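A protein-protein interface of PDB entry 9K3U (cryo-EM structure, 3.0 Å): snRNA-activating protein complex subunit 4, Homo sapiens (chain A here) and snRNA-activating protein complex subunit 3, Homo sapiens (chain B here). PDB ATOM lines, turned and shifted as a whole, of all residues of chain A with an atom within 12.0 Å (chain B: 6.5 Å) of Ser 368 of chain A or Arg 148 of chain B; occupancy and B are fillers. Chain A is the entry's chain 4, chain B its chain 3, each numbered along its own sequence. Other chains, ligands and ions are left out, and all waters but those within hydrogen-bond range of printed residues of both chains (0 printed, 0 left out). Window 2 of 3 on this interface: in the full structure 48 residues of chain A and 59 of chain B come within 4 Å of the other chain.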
ATOM      1  N   LEU A 357     -25.957  -6.770  13.716  1.00  0.00           N
ATOM      2  CA  LEU A 357     -25.093  -7.928  13.937  1.00  0.00           C
ATOM      3  C   LEU A 357     -25.760  -8.940  14.859  1.00  0.00           C
ATOM      4  O   LEU A 357     -25.593 -10.152  14.688  1.00  0.00           O
ATOM      5  CB  LEU A 357     -23.750  -7.480  14.512  1.00  0.00           C
ATOM      6  CG  LEU A 357     -22.632  -7.237  13.497  1.00  0.00           C
ATOM      7  CD1 LEU A 357     -23.078  -6.293  12.392  1.00  0.00           C
ATOM      8  CD2 LEU A 357     -21.392  -6.695  14.194  1.00  0.00           C
ATOM      9  N   THR A 358     -26.520  -8.462  15.847  1.00  0.00           N
ATOM     10  CA  THR A 358     -27.252  -9.378  16.718  1.00  0.00           C
ATOM     11  C   THR A 358     -28.312 -10.145  15.937  1.00  0.00           C
ATOM     12  O   THR A 358     -28.479 -11.357  16.124  1.00  0.00           O
ATOM     13  CB  THR A 358     -27.891  -8.606  17.873  1.00  0.00           C
ATOM     14  OG1 THR A 358     -26.882  -7.884  18.590  1.00  0.00           O
ATOM     15  CG2 THR A 358     -28.601  -9.560  18.825  1.00  0.00           C
ATOM     16  N   LEU A 360     -28.131 -10.849  12.812  1.00  0.00           N
ATOM     17  CA  LEU A 360     -27.382 -11.822  12.027  1.00  0.00           C
ATOM     18  C   LEU A 360     -27.011 -13.040  12.866  1.00  0.00           C
ATOM     19  O   LEU A 360     -27.170 -14.183  12.425  1.00  0.00           O
ATOM     20  CB  LEU A 360     -26.129 -11.176  11.435  1.00  0.00           C
ATOM     21  CG  LEU A 360     -26.289 -10.566  10.039  1.00  0.00           C
ATOM     22  CD1 LEU A 360     -27.167  -9.323  10.072  1.00  0.00           C
ATOM     23  CD2 LEU A 360     -24.931 -10.246   9.433  1.00  0.00           C
ATOM     24  N   VAL A 361     -26.521 -12.813  14.084  1.00  0.00           N
ATOM     25  CA  VAL A 361     -26.099 -13.887  14.976  1.00  0.00           C
ATOM     26  C   VAL A 361     -27.307 -14.714  15.404  1.00  0.00           C
ATOM     27  O   VAL A 361     -27.166 -15.865  15.829  1.00  0.00           O
ATOM     28  CB  VAL A 361     -25.357 -13.328  16.206  1.00  0.00           C
ATOM     29  CG1 VAL A 361     -25.121 -14.428  17.235  1.00  0.00           C
ATOM     30  CG2 VAL A 361     -24.043 -12.682  15.779  1.00  0.00           C
ATOM     31  N   GLN A 362     -28.498 -14.129  15.315  1.00  0.00           N
ATOM     32  CA  GLN A 362     -29.722 -14.847  15.645  1.00  0.00           C
ATOM     33  C   GLN A 362     -30.353 -15.570  14.465  1.00  0.00           C
ATOM     34  O   GLN A 362     -31.082 -16.544  14.692  1.00  0.00           O
ATOM     35  CB  GLN A 362     -30.767 -13.887  16.239  1.00  0.00           C
ATOM     36  CG  GLN A 362     -30.442 -13.395  17.645  1.00  0.00           C
ATOM     37  CD  GLN A 362     -30.314 -14.523  18.659  1.00  0.00           C
ATOM     38  OE1 GLN A 362     -29.476 -14.467  19.559  1.00  0.00           O
ATOM     39  NE2 GLN A 362     -31.148 -15.547  18.518  1.00  0.00           N
ATOM     40  N   GLU A 363     -30.104 -15.143  13.229  1.00  0.00           N
ATOM     41  CA  GLU A 363     -30.753 -15.756  12.075  1.00  0.00           C
ATOM     42  C   GLU A 363     -29.853 -16.730  11.322  1.00  0.00           C
ATOM     43  O   GLU A 363     -30.354 -17.732  10.798  1.00  0.00           O
ATOM     44  CB  GLU A 363     -31.236 -14.674  11.106  1.00  0.00           C
ATOM     45  CG  GLU A 363     -30.116 -13.930  10.399  1.00  0.00           C
ATOM     46  CD  GLU A 363     -30.621 -12.752   9.587  1.00  0.00           C
ATOM     47  OE1 GLU A 363     -31.850 -12.529   9.563  1.00  0.00           O
ATOM     48  OE2 GLU A 363     -29.788 -12.053   8.972  1.00  0.00           O
ATOM     49  N   MET A 364     -28.540 -16.471  11.256  1.00  0.00           N
ATOM     50  CA  MET A 364     -27.659 -17.297  10.438  1.00  0.00           C
ATOM     51  C   MET A 364     -26.498 -17.903  11.216  1.00  0.00           C
ATOM     52  O   MET A 364     -25.592 -18.474  10.594  1.00  0.00           O
ATOM     53  CB  MET A 364     -27.109 -16.480   9.259  1.00  0.00           C
ATOM     54  CG  MET A 364     -26.353 -15.224   9.665  1.00  0.00           C
ATOM     55  SD  MET A 364     -25.565 -14.398   8.269  1.00  0.00           S
ATOM     56  CE  MET A 364     -26.990 -13.982   7.265  1.00  0.00           C
ATOM     57  N   ARG A 365     -26.486 -17.805  12.544  1.00  0.00           N
ATOM     58  CA  ARG A 365     -25.432 -18.409  13.348  1.00  0.00           C
ATOM     59  C   ARG A 365     -25.822 -19.827  13.739  1.00  0.00           C
ATOM     60  O   ARG A 365     -27.006 -20.141  13.890  1.00  0.00           O
ATOM     61  CB  ARG A 365     -25.169 -17.577  14.606  1.00  0.00           C
ATOM     62  CG  ARG A 365     -23.990 -18.052  15.443  1.00  0.00           C
ATOM     63  CD  ARG A 365     -24.443 -18.912  16.614  1.00  0.00           C
ATOM     64  NE  ARG A 365     -25.330 -18.188  17.521  1.00  0.00           N
ATOM     65  CZ  ARG A 365     -25.985 -18.743  18.537  1.00  0.00           C
ATOM     66  NH1 ARG A 365     -25.860 -20.040  18.785  1.00  0.00           N
ATOM     67  NH2 ARG A 365     -26.769 -18.000  19.305  1.00  0.00           N
ATOM     68  N   VAL A 366     -24.817 -20.686  13.897  1.00  0.00           N
ATOM     69  CA  VAL A 366     -25.013 -22.082  14.271  1.00  0.00           C
ATOM     70  C   VAL A 366     -24.082 -22.380  15.436  1.00  0.00           C
ATOM     71  O   VAL A 366     -22.858 -22.435  15.266  1.00  0.00           O
ATOM     72  CB  VAL A 366     -24.747 -23.035  13.098  1.00  0.00           C
ATOM     73  CG1 VAL A 366     -25.128 -24.457  13.479  1.00  0.00           C
ATOM     74  CG2 VAL A 366     -25.512 -22.585  11.860  1.00  0.00           C
ATOM     75  N   GLY A 367     -24.658 -22.572  16.622  1.00  0.00           N
ATOM     76  CA  GLY A 367     -23.886 -22.958  17.787  1.00  0.00           C
ATOM     77  C   GLY A 367     -23.128 -21.807  18.416  1.00  0.00           C
ATOM     78  O   GLY A 367     -23.732 -20.822  18.853  1.00  0.00           O
ATOM     79  N   SER A 368     -21.803 -21.926  18.478  1.00  0.00           N
ATOM     80  CA  SER A 368     -20.948 -20.889  19.042  1.00  0.00           C
ATOM     81  C   SER A 368     -20.101 -20.173  18.002  1.00  0.00           C
ATOM     82  O   SER A 368     -19.842 -18.977  18.157  1.00  0.00           O
ATOM     83  CB  SER A 368     -20.019 -21.486  20.106  1.00  0.00           C
ATOM     84  OG  SER A 368     -19.103 -22.400  19.530  1.00  0.00           O
ATOM     85  N   HIS A 369     -19.668 -20.867  16.954  1.00  0.00           N
ATOM     86  CA  HIS A 369     -18.894 -20.225  15.903  1.00  0.00           C
ATOM     87  C   HIS A 369     -19.737 -19.167  15.201  1.00  0.00           C
ATOM     88  O   HIS A 369     -20.931 -19.365  14.955  1.00  0.00           O
ATOM     89  CB  HIS A 369     -18.406 -21.262  14.893  1.00  0.00           C
ATOM     90  CG  HIS A 369     -17.562 -20.690  13.797  1.00  0.00           C
ATOM     91  ND1 HIS A 369     -16.293 -20.198  14.014  1.00  0.00           N
ATOM     92  CD2 HIS A 369     -17.807 -20.530  12.473  1.00  0.00           C
ATOM     93  CE1 HIS A 369     -15.792 -19.761  12.871  1.00  0.00           C
ATOM     94  NE2 HIS A 369     -16.690 -19.951  11.922  1.00  0.00           N
ATOM     95  N   ILE A 370     -19.112 -18.041  14.881  1.00  0.00           N
ATOM     96  CA  ILE A 370     -19.778 -16.906  14.253  1.00  0.00           C
ATOM     97  C   ILE A 370     -19.110 -16.662  12.907  1.00  0.00           C
ATOM     98  O   ILE A 370     -17.884 -16.554  12.848  1.00  0.00           O
ATOM     99  CB  ILE A 370     -19.709 -15.635  15.119  1.00  0.00           C
ATOM    100  CG1 ILE A 370     -20.329 -15.898  16.495  1.00  0.00           C
ATOM    101  CG2 ILE A 370     -20.422 -14.480  14.420  1.00  0.00           C
ATOM    102  CD1 ILE A 370     -20.156 -14.757  17.478  1.00  0.00           C
ATOM    103  N   PRO A 371     -19.863 -16.571  11.805  1.00  0.00           N
ATOM    104  CA  PRO A 371     -19.234 -16.274  10.513  1.00  0.00           C
ATOM    105  C   PRO A 371     -18.868 -14.804  10.377  1.00  0.00           C
ATOM    106  O   PRO A 371     -19.626 -14.013   9.805  1.00  0.00           O
ATOM    107  CB  PRO A 371     -20.305 -16.690   9.500  1.00  0.00           C
ATOM    108  CG  PRO A 371     -21.589 -16.471  10.221  1.00  0.00           C
ATOM    109  CD  PRO A 371     -21.316 -16.791  11.668  1.00  0.00           C
ATOM    110  N   TYR A 372     -17.703 -14.428  10.914  1.00  0.00           N
ATOM    111  CA  TYR A 372     -17.290 -13.032  10.863  1.00  0.00           C
ATOM    112  C   TYR A 372     -17.179 -12.527   9.431  1.00  0.00           C
ATOM    113  O   TYR A 372     -17.366 -11.332   9.181  1.00  0.00           O
ATOM    114  CB  TYR A 372     -15.964 -12.848  11.601  1.00  0.00           C
ATOM    115  CG  TYR A 372     -16.121 -12.784  13.102  1.00  0.00           C
ATOM    116  CD1 TYR A 372     -16.537 -11.612  13.723  1.00  0.00           C
ATOM    117  CD2 TYR A 372     -15.872 -13.892  13.898  1.00  0.00           C
ATOM    118  CE1 TYR A 372     -16.691 -11.547  15.093  1.00  0.00           C
ATOM    119  CE2 TYR A 372     -16.020 -13.835  15.271  1.00  0.00           C
ATOM    120  CZ  TYR A 372     -16.429 -12.660  15.863  1.00  0.00           C
ATOM    121  OH  TYR A 372     -16.580 -12.597  17.228  1.00  0.00           O
ATOM    122  N   ARG A 373     -16.901 -13.413   8.473  1.00  0.00           N
ATOM    123  CA  ARG A 373     -16.892 -12.977   7.080  1.00  0.00           C
ATOM    124  C   ARG A 373     -18.296 -12.660   6.585  1.00  0.00           C
ATOM    125  O   ARG A 373     -18.483 -11.693   5.838  1.00  0.00           O
ATOM    126  CB  ARG A 373     -16.234 -14.037   6.194  1.00  0.00           C
ATOM    127  CG  ARG A 373     -14.708 -13.966   6.150  1.00  0.00           C
ATOM    128  CD  ARG A 373     -14.222 -12.600   5.671  1.00  0.00           C
ATOM    129  NE  ARG A 373     -12.832 -12.618   5.228  1.00  0.00           N
ATOM    130  CZ  ARG A 373     -12.193 -11.563   4.726  1.00  0.00           C
ATOM    131  NH1 ARG A 373     -10.927 -11.671   4.349  1.00  0.00           N
ATOM    132  NH2 ARG A 373     -12.820 -10.400   4.602  1.00  0.00           N
ATOM    133  N   ILE A 375     -20.534 -11.521   8.561  1.00  0.00           N
ATOM    134  CA  ILE A 375     -20.782 -10.247   9.232  1.00  0.00           C
ATOM    135  C   ILE A 375     -20.179  -9.100   8.432  1.00  0.00           C
ATOM    136  O   ILE A 375     -20.804  -8.048   8.255  1.00  0.00           O
ATOM    137  CB  ILE A 375     -20.224 -10.282  10.669  1.00  0.00           C
ATOM    138  CG1 ILE A 375     -20.883 -11.401  11.485  1.00  0.00           C
ATOM    139  CG2 ILE A 375     -20.417  -8.933  11.346  1.00  0.00           C
ATOM    140  CD1 ILE A 375     -22.383 -11.263  11.647  1.00  0.00           C
ATOM    141  N   LEU A 387     -12.796  -6.633  14.394  1.00  0.00           N
ATOM    142  CA  LEU A 387     -14.193  -7.016  14.561  1.00  0.00           C
ATOM    143  C   LEU A 387     -14.324  -8.220  15.481  1.00  0.00           C
ATOM    144  O   LEU A 387     -15.219  -8.263  16.332  1.00  0.00           O
ATOM    145  CB  LEU A 387     -14.833  -7.306  13.204  1.00  0.00           C
ATOM    146  CG  LEU A 387     -15.888  -6.292  12.759  1.00  0.00           C
ATOM    147  CD1 LEU A 387     -15.334  -4.874  12.799  1.00  0.00           C
ATOM    148  CD2 LEU A 387     -16.399  -6.630  11.368  1.00  0.00           C
ATOM    149  N   ILE A 388     -13.438  -9.204  15.334  1.00  0.00           N
ATOM    150  CA  ILE A 388     -13.460 -10.359  16.230  1.00  0.00           C
ATOM    151  C   ILE A 388     -13.259  -9.907  17.669  1.00  0.00           C
ATOM    152  O   ILE A 388     -14.083 -10.179  18.551  1.00  0.00           O
ATOM    153  CB  ILE A 388     -12.392 -11.386  15.811  1.00  0.00           C
ATOM    154  CG1 ILE A 388     -12.784 -12.050  14.490  1.00  0.00           C
ATOM    155  CG2 ILE A 388     -12.201 -12.430  16.905  1.00  0.00           C
ATOM    156  CD1 ILE A 388     -11.660 -12.828  13.836  1.00  0.00           C
ATOM    157  N   TRP A 391     -16.451  -7.699  18.863  1.00  0.00           N
ATOM    158  CA  TRP A 391     -17.746  -8.357  18.978  1.00  0.00           C
ATOM    159  C   TRP A 391     -17.714  -9.561  19.911  1.00  0.00           C
ATOM    160  O   TRP A 391     -18.768  -9.940  20.437  1.00  0.00           O
ATOM    161  CB  TRP A 391     -18.234  -8.789  17.593  1.00  0.00           C
ATOM    162  CG  TRP A 391     -19.521  -9.558  17.618  1.00  0.00           C
ATOM    163  CD1 TRP A 391     -19.666 -10.914  17.570  1.00  0.00           C
ATOM    164  CD2 TRP A 391     -20.846  -9.016  17.704  1.00  0.00           C
ATOM    165  NE1 TRP A 391     -20.998 -11.250  17.618  1.00  0.00           N
ATOM    166  CE2 TRP A 391     -21.744 -10.102  17.700  1.00  0.00           C
ATOM    167  CE3 TRP A 391     -21.361  -7.718  17.781  1.00  0.00           C
ATOM    168  CZ2 TRP A 391     -23.124  -9.933  17.770  1.00  0.00           C
ATOM    169  CZ3 TRP A 391     -22.733  -7.552  17.851  1.00  0.00           C
ATOM    170  CH2 TRP A 391     -23.599  -8.652  17.846  1.00  0.00           C
ATOM    171  N   THR A 392     -16.547 -10.171  20.136  1.00  0.00           N
ATOM    172  CA  THR A 392     -16.494 -11.322  21.032  1.00  0.00           C
ATOM    173  C   THR A 392     -16.853 -10.940  22.462  1.00  0.00           C
ATOM    174  O   THR A 392     -17.199 -11.810  23.269  1.00  0.00           O
ATOM    175  CB  THR A 392     -15.101 -11.955  20.987  1.00  0.00           C
ATOM    176  OG1 THR A 392     -14.779 -12.313  19.638  1.00  0.00           O
ATOM    177  CG2 THR A 392     -15.047 -13.202  21.862  1.00  0.00           C
ATOM    178  N   LYS A 393     -16.781  -9.654  22.796  1.00  0.00           N
ATOM    179  CA  LYS A 393     -17.011  -9.178  24.152  1.00  0.00           C
ATOM    180  C   LYS A 393     -18.050  -8.063  24.165  1.00  0.00           C
ATOM    181  O   LYS A 393     -18.217  -7.321  23.193  1.00  0.00           O
ATOM    182  CB  LYS A 393     -15.706  -8.673  24.779  1.00  0.00           C
ATOM    183  CG  LYS A 393     -14.499  -9.551  24.490  1.00  0.00           C
ATOM    184  CD  LYS A 393     -13.246  -9.008  25.157  1.00  0.00           C
ATOM    185  CE  LYS A 393     -11.999  -9.726  24.666  1.00  0.00           C
ATOM    186  NZ  LYS A 393     -12.086 -11.200  24.862  1.00  0.00           N
ATOM    187  N   ILE B 144      -3.842 -28.455  21.029  1.00  0.00           N
ATOM    188  CA  ILE B 144      -5.205 -27.960  21.197  1.00  0.00           C
ATOM    189  C   ILE B 144      -5.298 -27.253  22.541  1.00  0.00           C
ATOM    190  O   ILE B 144      -4.793 -27.749  23.558  1.00  0.00           O
ATOM    191  CB  ILE B 144      -6.219 -29.111  21.099  1.00  0.00           C
ATOM    192  CG1 ILE B 144      -5.931 -30.011  19.888  1.00  0.00           C
ATOM    193  CG2 ILE B 144      -7.635 -28.558  21.008  1.00  0.00           C
ATOM    194  CD1 ILE B 144      -6.008 -29.312  18.543  1.00  0.00           C
ATOM    195  N   THR B 145      -5.943 -26.087  22.558  1.00  0.00           N
ATOM    196  CA  THR B 145      -5.786 -25.170  23.693  1.00  0.00           C
ATOM    197  C   THR B 145      -6.834 -25.391  24.782  1.00  0.00           C
ATOM    198  O   THR B 145      -6.489 -25.760  25.907  1.00  0.00           O
ATOM    199  CB  THR B 145      -5.821 -23.721  23.199  1.00  0.00           C
ATOM    200  OG1 THR B 145      -4.921 -23.566  22.095  1.00  0.00           O
ATOM    201  CG2 THR B 145      -5.406 -22.776  24.316  1.00  0.00           C
ATOM    202  N   ILE B 146      -8.113 -25.170  24.468  1.00  0.00           N
ATOM    203  CA  ILE B 146      -9.116 -25.204  25.532  1.00  0.00           C
ATOM    204  C   ILE B 146     -10.275 -26.158  25.265  1.00  0.00           C
ATOM    205  O   ILE B 146     -10.316 -27.265  25.810  1.00  0.00           O
ATOM    206  CB  ILE B 146      -9.658 -23.779  25.759  1.00  0.00           C
ATOM    207  CG1 ILE B 146      -9.735 -23.022  24.426  1.00  0.00           C
ATOM    208  CG2 ILE B 146      -8.771 -23.022  26.728  1.00  0.00           C
ATOM    209  CD1 ILE B 146     -10.781 -21.936  24.383  1.00  0.00           C
ATOM    210  N   ASP B 147     -11.227 -25.743  24.411  1.00  0.00           N
ATOM    211  CA  ASP B 147     -12.350 -26.603  24.056  1.00  0.00           C
ATOM    212  C   ASP B 147     -12.879 -26.297  22.659  1.00  0.00           C
ATOM    213  O   ASP B 147     -14.032 -26.625  22.355  1.00  0.00           O
ATOM    214  CB  ASP B 147     -13.480 -26.464  25.086  1.00  0.00           C
ATOM    215  CG  ASP B 147     -14.388 -27.681  25.125  1.00  0.00           C
ATOM    216  OD1 ASP B 147     -14.420 -28.439  24.135  1.00  0.00           O
ATOM    217  OD2 ASP B 147     -15.073 -27.876  26.152  1.00  0.00           O
ATOM    218  N   ARG B 148     -12.072 -25.675  21.803  1.00  0.00           N
ATOM    219  CA  ARG B 148     -12.588 -25.003  20.620  1.00  0.00           C
ATOM    220  C   ARG B 148     -11.825 -25.491  19.392  1.00  0.00           C
ATOM    221  O   ARG B 148     -11.049 -26.451  19.458  1.00  0.00           O
ATOM    222  CB  ARG B 148     -12.510 -23.482  20.808  1.00  0.00           C
ATOM    223  CG  ARG B 148     -13.643 -22.908  21.648  1.00  0.00           C
ATOM    224  CD  ARG B 148     -14.820 -22.475  20.784  1.00  0.00           C
ATOM    225  NE  ARG B 148     -15.404 -23.579  20.030  1.00  0.00           N
ATOM    226  CZ  ARG B 148     -16.326 -23.431  19.082  1.00  0.00           C
ATOM    227  NH1 ARG B 148     -16.774 -22.221  18.768  1.00  0.00           N
ATOM    228  NH2 ARG B 148     -16.801 -24.492  18.446  1.00  0.00           N
ATOM    229  N   ALA B 149     -12.062 -24.820  18.262  1.00  0.00           N
ATOM    230  CA  ALA B 149     -11.631 -25.246  16.934  1.00  0.00           C
ATOM    231  C   ALA B 149     -12.509 -26.362  16.381  1.00  0.00           C
ATOM    232  O   ALA B 149     -12.180 -26.958  15.351  1.00  0.00           O
ATOM    233  CB  ALA B 149     -10.163 -25.689  16.926  1.00  0.00           C
ATOM    234  N   CYS B 150     -13.622 -26.651  17.050  1.00  0.00           N
ATOM    235  CA  CYS B 150     -14.549 -27.702  16.628  1.00  0.00           C
ATOM    236  C   CYS B 150     -15.739 -27.097  15.884  1.00  0.00           C
ATOM    237  O   CYS B 150     -16.901 -27.205  16.296  1.00  0.00           O
ATOM    238  CB  CYS B 150     -14.998 -28.509  17.842  1.00  0.00           C
ATOM    239  SG  CYS B 150     -15.863 -27.547  19.108  1.00  0.00           S
ATOM    240  N   ARG B 151     -15.433 -26.464  14.749  1.00  0.00           N
ATOM    241  CA  ARG B 151     -16.455 -25.751  13.988  1.00  0.00           C
ATOM    242  C   ARG B 151     -17.532 -26.703  13.478  1.00  0.00           C
ATOM    243  O   ARG B 151     -18.718 -26.549  13.803  1.00  0.00           O
ATOM    244  CB  ARG B 151     -15.804 -24.998  12.824  1.00  0.00           C
ATOM    245  CG  ARG B 151     -15.110 -23.710  13.237  1.00  0.00           C
ATOM    246  CD  ARG B 151     -14.636 -22.911  12.031  1.00  0.00           C
ATOM    247  NE  ARG B 151     -13.389 -23.426  11.473  1.00  0.00           N
ATOM    248  CZ  ARG B 151     -12.762 -22.893  10.425  1.00  0.00           C
ATOM    249  NH1 ARG B 151     -13.267 -21.829   9.815  1.00  0.00           N
ATOM    250  NH2 ARG B 151     -11.632 -23.427   9.988  1.00  0.00           N
ATOM    251  N   GLU B 153     -18.091 -29.677  14.318  1.00  0.00           N
ATOM    252  CA  GLU B 153     -18.690 -30.414  15.424  1.00  0.00           C
ATOM    253  C   GLU B 153     -19.834 -29.624  16.040  1.00  0.00           C
ATOM    254  O   GLU B 153     -20.941 -30.151  16.233  1.00  0.00           O
ATOM    255  CB  GLU B 153     -17.633 -30.731  16.478  1.00  0.00           C
ATOM    256  CG  GLU B 153     -16.317 -31.258  15.916  1.00  0.00           C
ATOM    257  CD  GLU B 153     -15.410 -31.831  16.990  1.00  0.00           C
ATOM    258  OE1 GLU B 153     -15.777 -31.757  18.182  1.00  0.00           O
ATOM    259  OE2 GLU B 153     -14.332 -32.354  16.642  1.00  0.00           O
ATOM    260  N   THR B 154     -19.590 -28.352  16.365  1.00  0.00           N
ATOM    261  CA  THR B 154     -20.655 -27.525  16.916  1.00  0.00           C
ATOM    262  C   THR B 154     -21.770 -27.305  15.900  1.00  0.00           C
ATOM    263  O   THR B 154     -22.943 -27.209  16.277  1.00  0.00           O
ATOM    264  CB  THR B 154     -20.097 -26.183  17.385  1.00  0.00           C
ATOM    265  OG1 THR B 154     -18.939 -26.401  18.200  1.00  0.00           O
ATOM    266  CG2 THR B 154     -21.139 -25.428  18.193  1.00  0.00           C
ATOM    267  N   PHE B 155     -21.426 -27.226  14.612  1.00  0.00           N
ATOM    268  CA  PHE B 155     -22.452 -27.133  13.579  1.00  0.00           C
ATOM    269  C   PHE B 155     -23.395 -28.325  13.643  1.00  0.00           C
ATOM    270  O   PHE B 155     -24.620 -28.164  13.678  1.00  0.00           O
ATOM    271  CB  PHE B 155     -21.807 -27.041  12.194  1.00  0.00           C
ATOM    272  CG  PHE B 155     -21.051 -25.762  11.945  1.00  0.00           C
ATOM    273  CD1 PHE B 155     -21.357 -24.601  12.635  1.00  0.00           C
ATOM    274  CD2 PHE B 155     -20.034 -25.725  11.003  1.00  0.00           C
ATOM    275  CE1 PHE B 155     -20.660 -23.432  12.394  1.00  0.00           C
ATOM    276  CE2 PHE B 155     -19.336 -24.560  10.761  1.00  0.00           C
ATOM    277  CZ  PHE B 155     -19.650 -23.412  11.457  1.00  0.00           C
ATOM    278  N   GLU B 158     -25.612 -28.232  16.844  1.00  0.00           N
ATOM    279  CA  GLU B 158     -26.729 -27.296  16.841  1.00  0.00           C
ATOM    280  C   GLU B 158     -27.785 -27.696  15.815  1.00  0.00           C
ATOM    281  O   GLU B 158     -28.987 -27.554  16.067  1.00  0.00           O
ATOM    282  CB  GLU B 158     -26.232 -25.876  16.573  1.00  0.00           C
ATOM    283  CG  GLU B 158     -27.056 -24.796  17.265  1.00  0.00           C
ATOM    284  CD  GLU B 158     -27.583 -23.741  16.307  1.00  0.00           C
ATOM    285  OE1 GLU B 158     -27.886 -24.080  15.146  1.00  0.00           O
ATOM    286  OE2 GLU B 158     -27.694 -22.568  16.723  1.00  0.00           O
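NH1 of Arg 148 of chain B is in hydrogen-bond range of OG of Ser 368 of chain A.
The guanidinium group (NH1) of Arg 365 of chain A lies within salt-bridge range of the side-chain carboxylate (OE2) of Glu 158 of chain B (3.7 Å).
The backbone NH (N) of Gly 367 of chain A is in hydrogen-bond range of the side-chain carboxylate (OE2) of Glu 158 of chain B.
SG of Cys 150 of chain B is in hydrogen-bond range of NH2 of Arg 148 of chain B.
The guanidinium group (NH2) of Arg 148 of chain B is in hydrogen-bond range of the side-chain hydroxyl (OG1) of Thr 154 of chain B, 2.9 Å away.
The backbone carbonyl oxygen (O) of Cys 150 of chain B sits at hydrogen-bond distance from the side-chain hydroxyl (OG1) of Thr 154 of chain B, at 2.9 Å.
The guanidinium group (NE) of Arg 365 of chain A lies close to the backbone carbonyl oxygen (O) of Val 361 of chain A (3.4 Å).
The backbone carbonyl oxygen (O) of Gly 367 of chain A lies close to the guanidinium group (NE) of Arg 365 of chain A (3.4 Å).
Among the printed residues, merely in contact across the chains: Val 366 of chain A with Phe 155 of chain B (3.7 Å), Val 366 of chain A with Glu 158 of chain B (3.2 Å), Gly 367 of chain A with Thr 154 of chain B (3.7 Å), Ser 368 of chain A with Thr 154 of chain B (3.6 Å), His 369 of chain A with Arg 148 of chain B (3.7 Å), His 369 of chain A with Arg 151 of chain B (3.5 Å) and His 369 of chain A with Phe 155 of chain B (3.6 Å).
Leu 360 of chain A touches none of the printed residues of chain B.
Of the printed residues of chain B, Arg 365 of chain A touches Glu 158.
Printed residues of chain B within 4 Å of Val 366 of chain A: Phe 155 (3.7 Å) and Glu 158 (3.2 Å).
Ser 368 of chain A touches just these residues of chain B: Arg 148 and Thr 154.
Printed residues of chain B within 4 Å of His 369 of chain A: Arg 148 (3.7 Å), Arg 151 (3.5 Å) and Phe 155 (3.6 Å).
Arg 148 of chain B touches just these residues of chain A: Ser 368 (2.5 Å) and His 369 (3.7 Å).
No residue of chain A comes within 4 Å of Ala 149 of chain B.
No residue of chain A comes within 4 Å of Cys 150 of chain B.
No residue of chain A comes within 4 Å of Glu 153 of chain B.
Of chain A, only Gly 367 (3.7 Å) and Ser 368 (3.6 Å) come within 4 Å of Thr 154 of chain B.
The nearest residue of chain A that does not touch Arg 148 of chain B is Ile 370 of chain A (6.2 Å).
The nearest printed residue of chain B that does not touch Val 366 of chain A is Thr 154 of chain B (4.5 Å).
Hydrophobic or aromatic side chains of chain B that line the printed part of chain A: Phe 155.
Hydrophobic or aromatic side chains of chain A within 4 Å of the printed part of chain B: Val 366 and His 369.
Among the printed residues, Asp or Glu carboxylates within 4 Å of a Lys or Arg side-chain nitrogen of the other chain: Arg 365 of chain A with Glu 158 of chain B (3.7 Å).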
